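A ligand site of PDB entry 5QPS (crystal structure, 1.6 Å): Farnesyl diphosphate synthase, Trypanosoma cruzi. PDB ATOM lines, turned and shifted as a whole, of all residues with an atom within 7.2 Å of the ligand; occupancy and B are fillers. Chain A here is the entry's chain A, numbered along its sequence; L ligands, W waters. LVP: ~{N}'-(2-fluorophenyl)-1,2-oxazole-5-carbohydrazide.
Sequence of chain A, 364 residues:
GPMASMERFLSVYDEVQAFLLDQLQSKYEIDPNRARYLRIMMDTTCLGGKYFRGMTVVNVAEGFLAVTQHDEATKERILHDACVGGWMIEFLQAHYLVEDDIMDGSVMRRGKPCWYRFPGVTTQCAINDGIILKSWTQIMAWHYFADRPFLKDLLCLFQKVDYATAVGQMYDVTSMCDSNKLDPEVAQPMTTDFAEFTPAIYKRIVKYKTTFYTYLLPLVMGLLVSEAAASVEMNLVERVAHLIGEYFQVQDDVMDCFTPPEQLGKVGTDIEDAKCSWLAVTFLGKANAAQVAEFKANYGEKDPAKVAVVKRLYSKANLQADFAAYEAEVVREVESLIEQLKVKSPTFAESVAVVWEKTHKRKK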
ATOM      1  N   PHE A 197     -14.789 -20.433 -18.399  1.00  0.00           N
ATOM      2  CA  PHE A 197     -13.763 -19.510 -18.081  1.00  0.00           C
ATOM      3  C   PHE A 197     -12.469 -20.024 -18.675  1.00  0.00           C
ATOM      4  O   PHE A 197     -11.652 -20.623 -17.956  1.00  0.00           O
ATOM      5  CB  PHE A 197     -13.643 -19.364 -16.632  1.00  0.00           C
ATOM      6  CG  PHE A 197     -14.599 -18.338 -15.999  1.00  0.00           C
ATOM      7  CD1 PHE A 197     -15.969 -18.272 -16.358  1.00  0.00           C
ATOM      8  CD2 PHE A 197     -14.138 -17.499 -15.063  1.00  0.00           C
ATOM      9  CE1 PHE A 197     -16.841 -17.326 -15.776  1.00  0.00           C
ATOM     10  CE2 PHE A 197     -14.989 -16.596 -14.422  1.00  0.00           C
ATOM     11  CZ  PHE A 197     -16.331 -16.475 -14.820  1.00  0.00           C
ATOM     12  N   THR A 198     -12.299 -19.862 -20.010  1.00  0.00           N
ATOM     13  CA  THR A 198     -11.087 -20.302 -20.695  1.00  0.00           C
ATOM     14  C   THR A 198     -10.380 -19.129 -21.373  1.00  0.00           C
ATOM     15  O   THR A 198     -11.004 -18.095 -21.544  1.00  0.00           O
ATOM     16  CB  THR A 198     -11.388 -21.334 -21.785  1.00  0.00           C
ATOM     17  OG1 THR A 198     -12.206 -20.786 -22.810  1.00  0.00           O
ATOM     18  CG2 THR A 198     -12.194 -22.570 -21.198  1.00  0.00           C
ATOM     19  N   PRO A 199      -9.155 -19.304 -21.803  1.00  0.00           N
ATOM     20  CA  PRO A 199      -8.452 -18.212 -22.487  1.00  0.00           C
ATOM     21  C   PRO A 199      -9.200 -17.934 -23.806  1.00  0.00           C
ATOM     22  O   PRO A 199      -9.427 -16.785 -24.110  1.00  0.00           O
ATOM     23  CB  PRO A 199      -7.069 -18.825 -22.725  1.00  0.00           C
ATOM     24  CG  PRO A 199      -6.898 -19.667 -21.540  1.00  0.00           C
ATOM     25  CD  PRO A 199      -8.188 -20.333 -21.342  1.00  0.00           C
ATOM     26  N   ALA A 200      -9.619 -18.947 -24.533  1.00  0.00           N
ATOM     27  CA  ALA A 200     -10.315 -18.681 -25.817  1.00  0.00           C
ATOM     28  C   ALA A 200     -11.620 -17.904 -25.642  1.00  0.00           C
ATOM     29  O   ALA A 200     -11.897 -17.003 -26.406  1.00  0.00           O
ATOM     30  CB  ALA A 200     -10.547 -19.955 -26.572  1.00  0.00           C
ATOM     31  N   TYR A 202     -12.410 -15.970 -23.051  1.00  0.00           N
ATOM     32  CA  TYR A 202     -12.047 -14.677 -22.599  1.00  0.00           C
ATOM     33  C   TYR A 202     -11.631 -13.783 -23.847  1.00  0.00           C
ATOM     34  O   TYR A 202     -12.031 -12.624 -23.940  1.00  0.00           O
ATOM     35  CB  TYR A 202     -10.848 -14.741 -21.629  1.00  0.00           C
ATOM     36  CG  TYR A 202     -10.281 -13.391 -21.200  1.00  0.00           C
ATOM     37  CD1 TYR A 202     -10.860 -12.713 -20.204  1.00  0.00           C
ATOM     38  CD2 TYR A 202      -9.213 -12.819 -21.855  1.00  0.00           C
ATOM     39  CE1 TYR A 202     -10.350 -11.524 -19.738  1.00  0.00           C
ATOM     40  CE2 TYR A 202      -8.703 -11.579 -21.440  1.00  0.00           C
ATOM     41  CZ  TYR A 202      -9.309 -10.962 -20.361  1.00  0.00           C
ATOM     42  OH  TYR A 202      -8.851  -9.755 -19.895  1.00  0.00           O
ATOM     43  N   LYS A 203     -10.786 -14.324 -24.702  1.00  0.00           N
ATOM     44  CA  LYS A 203     -10.313 -13.646 -25.918  1.00  0.00           C
ATOM     45  C   LYS A 203     -11.528 -13.174 -26.747  1.00  0.00           C
ATOM     46  O   LYS A 203     -11.484 -12.068 -27.221  1.00  0.00           O
ATOM     47  CB  LYS A 203      -9.373 -14.536 -26.798  1.00  0.00           C
ATOM     48  CG  LYS A 203      -8.039 -14.796 -26.099  1.00  0.00           C
ATOM     49  CD  LYS A 203      -7.054 -15.744 -26.814  1.00  0.00           C
ATOM     50  CE  LYS A 203      -5.814 -15.789 -25.917  1.00  0.00           C
ATOM     51  NZ  LYS A 203      -4.698 -16.648 -26.416  1.00  0.00           N
ATOM     52  N   GLU A 246      -6.291  -6.771 -26.391  1.00  0.00           N
ATOM     53  CA  GLU A 246      -6.476  -7.820 -25.359  1.00  0.00           C
ATOM     54  C   GLU A 246      -5.600  -7.526 -24.138  1.00  0.00           C
ATOM     55  O   GLU A 246      -6.016  -7.600 -22.995  1.00  0.00           O
ATOM     56  CB  GLU A 246      -6.144  -9.179 -25.937  1.00  0.00           C
ATOM     57  CG  GLU A 246      -6.507 -10.277 -25.007  1.00  0.00           C
ATOM     58  CD  GLU A 246      -6.129 -11.618 -25.607  1.00  0.00           C
ATOM     59  OE1 GLU A 246      -5.182 -12.301 -25.090  1.00  0.00           O
ATOM     60  OE2 GLU A 246      -6.732 -11.956 -26.640  1.00  0.00           O
ATOM     61  N   VAL A 250      -6.496  -7.083 -20.177  1.00  0.00           N
ATOM     62  CA  VAL A 250      -5.843  -7.819 -19.107  1.00  0.00           C
ATOM     63  C   VAL A 250      -5.352  -6.932 -17.982  1.00  0.00           C
ATOM     64  O   VAL A 250      -5.611  -7.200 -16.793  1.00  0.00           O
ATOM     65  CB  VAL A 250      -4.721  -8.738 -19.647  1.00  0.00           C
ATOM     66  CG1 VAL A 250      -3.890  -9.310 -18.491  1.00  0.00           C
ATOM     67  CG2 VAL A 250      -5.317  -9.816 -20.505  1.00  0.00           C
ATOM     68  N   SER A 277     -12.760 -12.679 -15.931  1.00  0.00           N
ATOM     69  CA  SER A 277     -11.594 -11.777 -15.957  1.00  0.00           C
ATOM     70  C   SER A 277     -10.348 -12.601 -16.203  1.00  0.00           C
ATOM     71  O   SER A 277     -10.370 -13.837 -16.031  1.00  0.00           O
ATOM     72  CB  SER A 277     -11.456 -11.110 -14.634  1.00  0.00           C
ATOM     73  OG  SER A 277     -11.104 -12.125 -13.708  1.00  0.00           O
ATOM     74  N   TRP A 278      -9.263 -11.944 -16.636  1.00  0.00           N
ATOM     75  CA  TRP A 278      -8.008 -12.629 -16.826  1.00  0.00           C
ATOM     76  C   TRP A 278      -7.516 -13.353 -15.514  1.00  0.00           C
ATOM     77  O   TRP A 278      -6.956 -14.437 -15.579  1.00  0.00           O
ATOM     78  CB  TRP A 278      -6.940 -11.651 -17.281  1.00  0.00           C
ATOM     79  CG  TRP A 278      -5.607 -12.287 -17.504  1.00  0.00           C
ATOM     80  CD1 TRP A 278      -5.153 -12.874 -18.661  1.00  0.00           C
ATOM     81  CD2 TRP A 278      -4.544 -12.369 -16.559  1.00  0.00           C
ATOM     82  NE1 TRP A 278      -3.895 -13.356 -18.454  1.00  0.00           N
ATOM     83  CE2 TRP A 278      -3.498 -13.040 -17.170  1.00  0.00           C
ATOM     84  CE3 TRP A 278      -4.390 -11.936 -15.224  1.00  0.00           C
ATOM     85  CZ2 TRP A 278      -2.284 -13.331 -16.508  1.00  0.00           C
ATOM     86  CZ3 TRP A 278      -3.190 -12.215 -14.564  1.00  0.00           C
ATOM     87  CH2 TRP A 278      -2.152 -12.902 -15.226  1.00  0.00           C
ATOM     88  N   LEU A 279      -7.728 -12.684 -14.389  1.00  0.00           N
ATOM     89  CA  LEU A 279      -7.377 -13.258 -13.127  1.00  0.00           C
ATOM     90  C   LEU A 279      -8.095 -14.579 -12.920  1.00  0.00           C
ATOM     91  O   LEU A 279      -7.480 -15.584 -12.594  1.00  0.00           O
ATOM     92  CB  LEU A 279      -7.717 -12.306 -11.967  1.00  0.00           C
ATOM     93  CG  LEU A 279      -6.851 -11.049 -11.924  1.00  0.00           C
ATOM     94  CD1 LEU A 279      -7.499  -9.973 -11.043  1.00  0.00           C
ATOM     95  CD2 LEU A 279      -5.433 -11.353 -11.513  1.00  0.00           C
ATOM     96  N   ALA A 280      -9.413 -14.578 -13.114  1.00  0.00           N
ATOM     97  CA  ALA A 280     -10.191 -15.817 -12.816  1.00  0.00           C
ATOM     98  C   ALA A 280      -9.787 -16.934 -13.773  1.00  0.00           C
ATOM     99  O   ALA A 280      -9.599 -18.102 -13.409  1.00  0.00           O
ATOM    100  CB  ALA A 280     -11.679 -15.552 -12.901  1.00  0.00           C
ATOM    101  N   VAL A 281      -9.642 -16.583 -15.057  1.00  0.00           N
ATOM    102  CA  VAL A 281      -9.236 -17.571 -16.065  1.00  0.00           C
ATOM    103  C   VAL A 281      -7.864 -18.178 -15.734  1.00  0.00           C
ATOM    104  O   VAL A 281      -7.652 -19.447 -15.787  1.00  0.00           O
ATOM    105  CB  VAL A 281      -9.276 -17.000 -17.506  1.00  0.00           C
ATOM    106  CG1 VAL A 281      -8.829 -18.005 -18.523  1.00  0.00           C
ATOM    107  CG2 VAL A 281     -10.726 -16.594 -17.802  1.00  0.00           C
ATOM    108  N   THR A 282      -6.956 -17.269 -15.453  1.00  0.00           N
ATOM    109  CA  THR A 282      -5.540 -17.654 -15.247  1.00  0.00           C
ATOM    110  C   THR A 282      -5.453 -18.510 -13.945  1.00  0.00           C
ATOM    111  O   THR A 282      -4.746 -19.536 -13.913  1.00  0.00           O
ATOM    112  CB  THR A 282      -4.678 -16.443 -15.183  1.00  0.00           C
ATOM    113  OG1 THR A 282      -4.791 -15.747 -16.465  1.00  0.00           O
ATOM    114  CG2 THR A 282      -3.225 -16.809 -14.930  1.00  0.00           C
ATOM    115  N   PHE A 283      -6.200 -18.073 -12.933  1.00  0.00           N
ATOM    116  CA  PHE A 283      -6.293 -18.820 -11.671  1.00  0.00           C
ATOM    117  C   PHE A 283      -6.773 -20.234 -11.887  1.00  0.00           C
ATOM    118  O   PHE A 283      -6.120 -21.243 -11.484  1.00  0.00           O
ATOM    119  CB  PHE A 283      -7.147 -18.098 -10.663  1.00  0.00           C
ATOM    120  CG  PHE A 283      -7.322 -18.887  -9.384  1.00  0.00           C
ATOM    121  CD1 PHE A 283      -6.367 -18.812  -8.391  1.00  0.00           C
ATOM    122  CD2 PHE A 283      -8.445 -19.765  -9.224  1.00  0.00           C
ATOM    123  CE1 PHE A 283      -6.534 -19.561  -7.197  1.00  0.00           C
ATOM    124  CE2 PHE A 283      -8.592 -20.529  -8.070  1.00  0.00           C
ATOM    125  CZ  PHE A 283      -7.638 -20.389  -7.043  1.00  0.00           C
ATOM    126  N   GLY A 285      -6.717 -21.893 -14.546  1.00  0.00           N
ATOM    127  CA  GLY A 285      -5.768 -22.616 -15.377  1.00  0.00           C
ATOM    128  C   GLY A 285      -4.570 -23.167 -14.642  1.00  0.00           C
ATOM    129  O   GLY A 285      -3.767 -23.902 -15.208  1.00  0.00           O
ATOM    130  N   LYS A 286      -4.417 -22.821 -13.378  1.00  0.00           N
ATOM    131  CA  LYS A 286      -3.247 -23.393 -12.668  1.00  0.00           C
ATOM    132  C   LYS A 286      -3.596 -23.970 -11.294  1.00  0.00           C
ATOM    133  O   LYS A 286      -2.750 -24.584 -10.684  1.00  0.00           O
ATOM    134  CB  LYS A 286      -2.184 -22.305 -12.510  1.00  0.00           C
ATOM    135  CG  LYS A 286      -2.494 -21.240 -11.498  1.00  0.00           C
ATOM    136  CD  LYS A 286      -1.443 -20.133 -11.599  1.00  0.00           C
ATOM    137  CE  LYS A 286       0.009 -20.534 -11.374  1.00  0.00           C
ATOM    138  NZ  LYS A 286       0.705 -19.210 -11.149  1.00  0.00           N
ATOM    139  N   LEU A 319      -0.040 -14.885  -9.572  1.00  0.00           N
ATOM    140  CA  LEU A 319      -0.567 -14.500 -10.891  1.00  0.00           C
ATOM    141  C   LEU A 319       0.351 -13.481 -11.551  1.00  0.00           C
ATOM    142  O   LEU A 319       0.451 -13.479 -12.751  1.00  0.00           O
ATOM    143  CB  LEU A 319      -2.031 -13.994 -10.762  1.00  0.00           C
ATOM    144  CG  LEU A 319      -2.959 -15.139 -10.351  1.00  0.00           C
ATOM    145  CD1 LEU A 319      -4.393 -14.654 -10.274  1.00  0.00           C
ATOM    146  CD2 LEU A 319      -2.935 -16.350 -11.250  1.00  0.00           C
ATOM    147  N   ALA A 321       3.409 -13.845 -11.922  1.00  0.00           N
ATOM    148  CA  ALA A 321       4.296 -14.659 -12.803  1.00  0.00           C
ATOM    149  C   ALA A 321       3.650 -14.946 -14.143  1.00  0.00           C
ATOM    150  O   ALA A 321       4.292 -14.951 -15.197  1.00  0.00           O
ATOM    151  CB  ALA A 321       4.698 -16.011 -12.165  1.00  0.00           C
ATOM    152  N   ASP A 322       2.355 -15.239 -14.101  1.00  0.00           N
ATOM    153  CA  ASP A 322       1.681 -15.517 -15.288  1.00  0.00           C
ATOM    154  C   ASP A 322       1.548 -14.209 -16.081  1.00  0.00           C
ATOM    155  O   ASP A 322       1.630 -14.304 -17.296  1.00  0.00           O
ATOM    156  CB  ASP A 322       0.301 -16.108 -15.031  1.00  0.00           C
ATOM    157  CG  ASP A 322       0.373 -17.456 -14.353  1.00  0.00           C
ATOM    158  OD1 ASP A 322       0.325 -17.411 -13.118  1.00  0.00           O
ATOM    159  OD2 ASP A 322       0.481 -18.473 -15.087  1.00  0.00           O
ATOM    160  N   PHE A 323       1.288 -13.057 -15.420  1.00  0.00           N
ATOM    161  CA  PHE A 323       1.127 -11.769 -16.145  1.00  0.00           C
ATOM    162  C   PHE A 323       2.426 -11.446 -16.858  1.00  0.00           C
ATOM    163  O   PHE A 323       2.436 -11.102 -18.018  1.00  0.00           O
ATOM    164  CB  PHE A 323       0.777 -10.618 -15.253  1.00  0.00           C
ATOM    165  CG  PHE A 323       0.643  -9.321 -16.011  1.00  0.00           C
ATOM    166  CD1 PHE A 323      -0.510  -9.013 -16.715  1.00  0.00           C
ATOM    167  CD2 PHE A 323       1.729  -8.410 -16.084  1.00  0.00           C
ATOM    168  CE1 PHE A 323      -0.596  -7.833 -17.415  1.00  0.00           C
ATOM    169  CE2 PHE A 323       1.628  -7.222 -16.821  1.00  0.00           C
ATOM    170  CZ  PHE A 323       0.460  -6.936 -17.463  1.00  0.00           C
ATOM    171  N   ALA A 324       3.547 -11.657 -16.167  1.00  0.00           N
ATOM    172  CA  ALA A 324       4.850 -11.375 -16.801  1.00  0.00           C
ATOM    173  C   ALA A 324       5.036 -12.227 -18.048  1.00  0.00           C
ATOM    174  O   ALA A 324       5.555 -11.746 -19.040  1.00  0.00           O
ATOM    175  CB  ALA A 324       6.012 -11.580 -15.804  1.00  0.00           C
ATOM    176  N   ALA A 325       4.669 -13.520 -18.007  1.00  0.00           N
ATOM    177  CA  ALA A 325       4.798 -14.389 -19.162  1.00  0.00           C
ATOM    178  C   ALA A 325       3.849 -13.988 -20.296  1.00  0.00           C
ATOM    179  O   ALA A 325       4.249 -14.016 -21.505  1.00  0.00           O
ATOM    180  CB  ALA A 325       4.574 -15.851 -18.836  1.00  0.00           C
ATOM    181  N   TYR A 326       2.607 -13.660 -19.913  1.00  0.00           N
ATOM    182  CA  TYR A 326       1.600 -13.189 -20.871  1.00  0.00           C
ATOM    183  C   TYR A 326       2.193 -11.951 -21.565  1.00  0.00           C
ATOM    184  O   TYR A 326       2.228 -11.860 -22.796  1.00  0.00           O
ATOM    185  CB  TYR A 326       0.277 -12.881 -20.156  1.00  0.00           C
ATOM    186  CG  TYR A 326      -0.779 -12.323 -21.071  1.00  0.00           C
ATOM    187  CD1 TYR A 326      -1.668 -13.146 -21.687  1.00  0.00           C
ATOM    188  CD2 TYR A 326      -0.846 -10.977 -21.343  1.00  0.00           C
ATOM    189  CE1 TYR A 326      -2.625 -12.635 -22.553  1.00  0.00           C
ATOM    190  CE2 TYR A 326      -1.777 -10.469 -22.219  1.00  0.00           C
ATOM    191  CZ  TYR A 326      -2.672 -11.309 -22.807  1.00  0.00           C
ATOM    192  OH  TYR A 326      -3.612 -10.846 -23.712  1.00  0.00           O
ATOM    193  N   GLU A 327       2.674 -11.021 -20.756  1.00  0.00           N
ATOM    194  CA  GLU A 327       3.205  -9.770 -21.230  1.00  0.00           C
ATOM    195  C   GLU A 327       4.419  -9.902 -22.148  1.00  0.00           C
ATOM    196  O   GLU A 327       4.505  -9.235 -23.216  1.00  0.00           O
ATOM    197  CB  GLU A 327       3.572  -8.943 -20.015  1.00  0.00           C
ATOM    198  CG  GLU A 327       4.174  -7.631 -20.409  1.00  0.00           C
ATOM    199  CD  GLU A 327       4.793  -6.887 -19.286  1.00  0.00           C
ATOM    200  OE1 GLU A 327       4.983  -7.475 -18.224  1.00  0.00           O
ATOM    201  OE2 GLU A 327       5.110  -5.721 -19.488  1.00  0.00           O
HETATM  202  N1  LVP L   1      -3.087 -17.517 -18.898  1.00  0.00           N
HETATM  203  C4  LVP L   1      -4.834 -16.427 -20.243  1.00  0.00           C
HETATM  204  C5  LVP L   1      -4.096 -16.502 -21.441  1.00  0.00           C
HETATM  205  C6  LVP L   1      -1.915 -16.732 -18.949  1.00  0.00           C
HETATM  206  C7  LVP L   1      -0.678 -17.497 -18.770  1.00  0.00           C
HETATM  207  C8  LVP L   1       0.626 -17.083 -18.784  1.00  0.00           C
HETATM  208  N   LVP L   1      -4.381 -16.990 -18.960  1.00  0.00           N
HETATM  209  C   LVP L   1      -4.604 -15.846 -22.604  1.00  0.00           C
HETATM  210  O   LVP L   1      -1.896 -15.507 -19.165  1.00  0.00           O
HETATM  211  C1  LVP L   1      -5.854 -15.185 -22.506  1.00  0.00           C
HETATM  212  C2  LVP L   1      -6.521 -15.160 -21.348  1.00  0.00           C
HETATM  213  C3  LVP L   1      -6.027 -15.750 -20.237  1.00  0.00           C
HETATM  214  C9  LVP L   1       1.395 -18.297 -18.583  1.00  0.00           C
HETATM  215  F   LVP L   1      -6.660 -15.607 -19.048  1.00  0.00           F
HETATM  216  N2  LVP L   1       0.542 -19.323 -18.492  1.00  0.00           N
HETATM  217  O1  LVP L   1      -0.723 -18.846 -18.599  1.00  0.00           O
HETATM  218  O   HOH W   1      -3.657 -20.566 -18.467  1.00  0.00           O
HETATM  219  O   HOH W   2      -0.736 -22.165 -18.439  1.00  0.00           O
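Residues that only touch the ligand: Val 281 (3.3 Å), Asp 322 (3.3 Å), Tyr 326 (3.5 Å), Lys 203 (3.5 Å), Tyr 202 (3.6 Å), Pro 199 (3.8 Å) and Glu 246 (3.9 Å). Hydrophobic or aromatic side chains within 4 Å of the ligand: Pro 199, Tyr 202, Trp 278, Val 281 and Tyr 326. Within 4 Å of the ligand: Pro 199, Tyr 202, Lys 203, Glu 246, Trp 278, Val 281, Thr 282, Asp 322 and Tyr 326. Along chain A the residues within 4 Å of the ligand span positions 199 to 326.
The side-chain hydroxyl (OG1) of Thr 282 is in hydrogen-bond range of a nitrogen (N) of the ligand. NE1 of Trp 278 is in hydrogen-bond range of O of the ligand, at 3.0 Å.
O of Trp 278 sits at hydrogen-bond distance from OG1 of Thr 282 (2.7 Å). NZ of Lys 286 lies within salt-bridge range of OD1 of Asp 322 (2.7 Å). The side-chain hydroxyl of Tyr 326 lies within hydrogen-bond range of the side-chain carboxylate of Glu 246 (2.5 Å).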
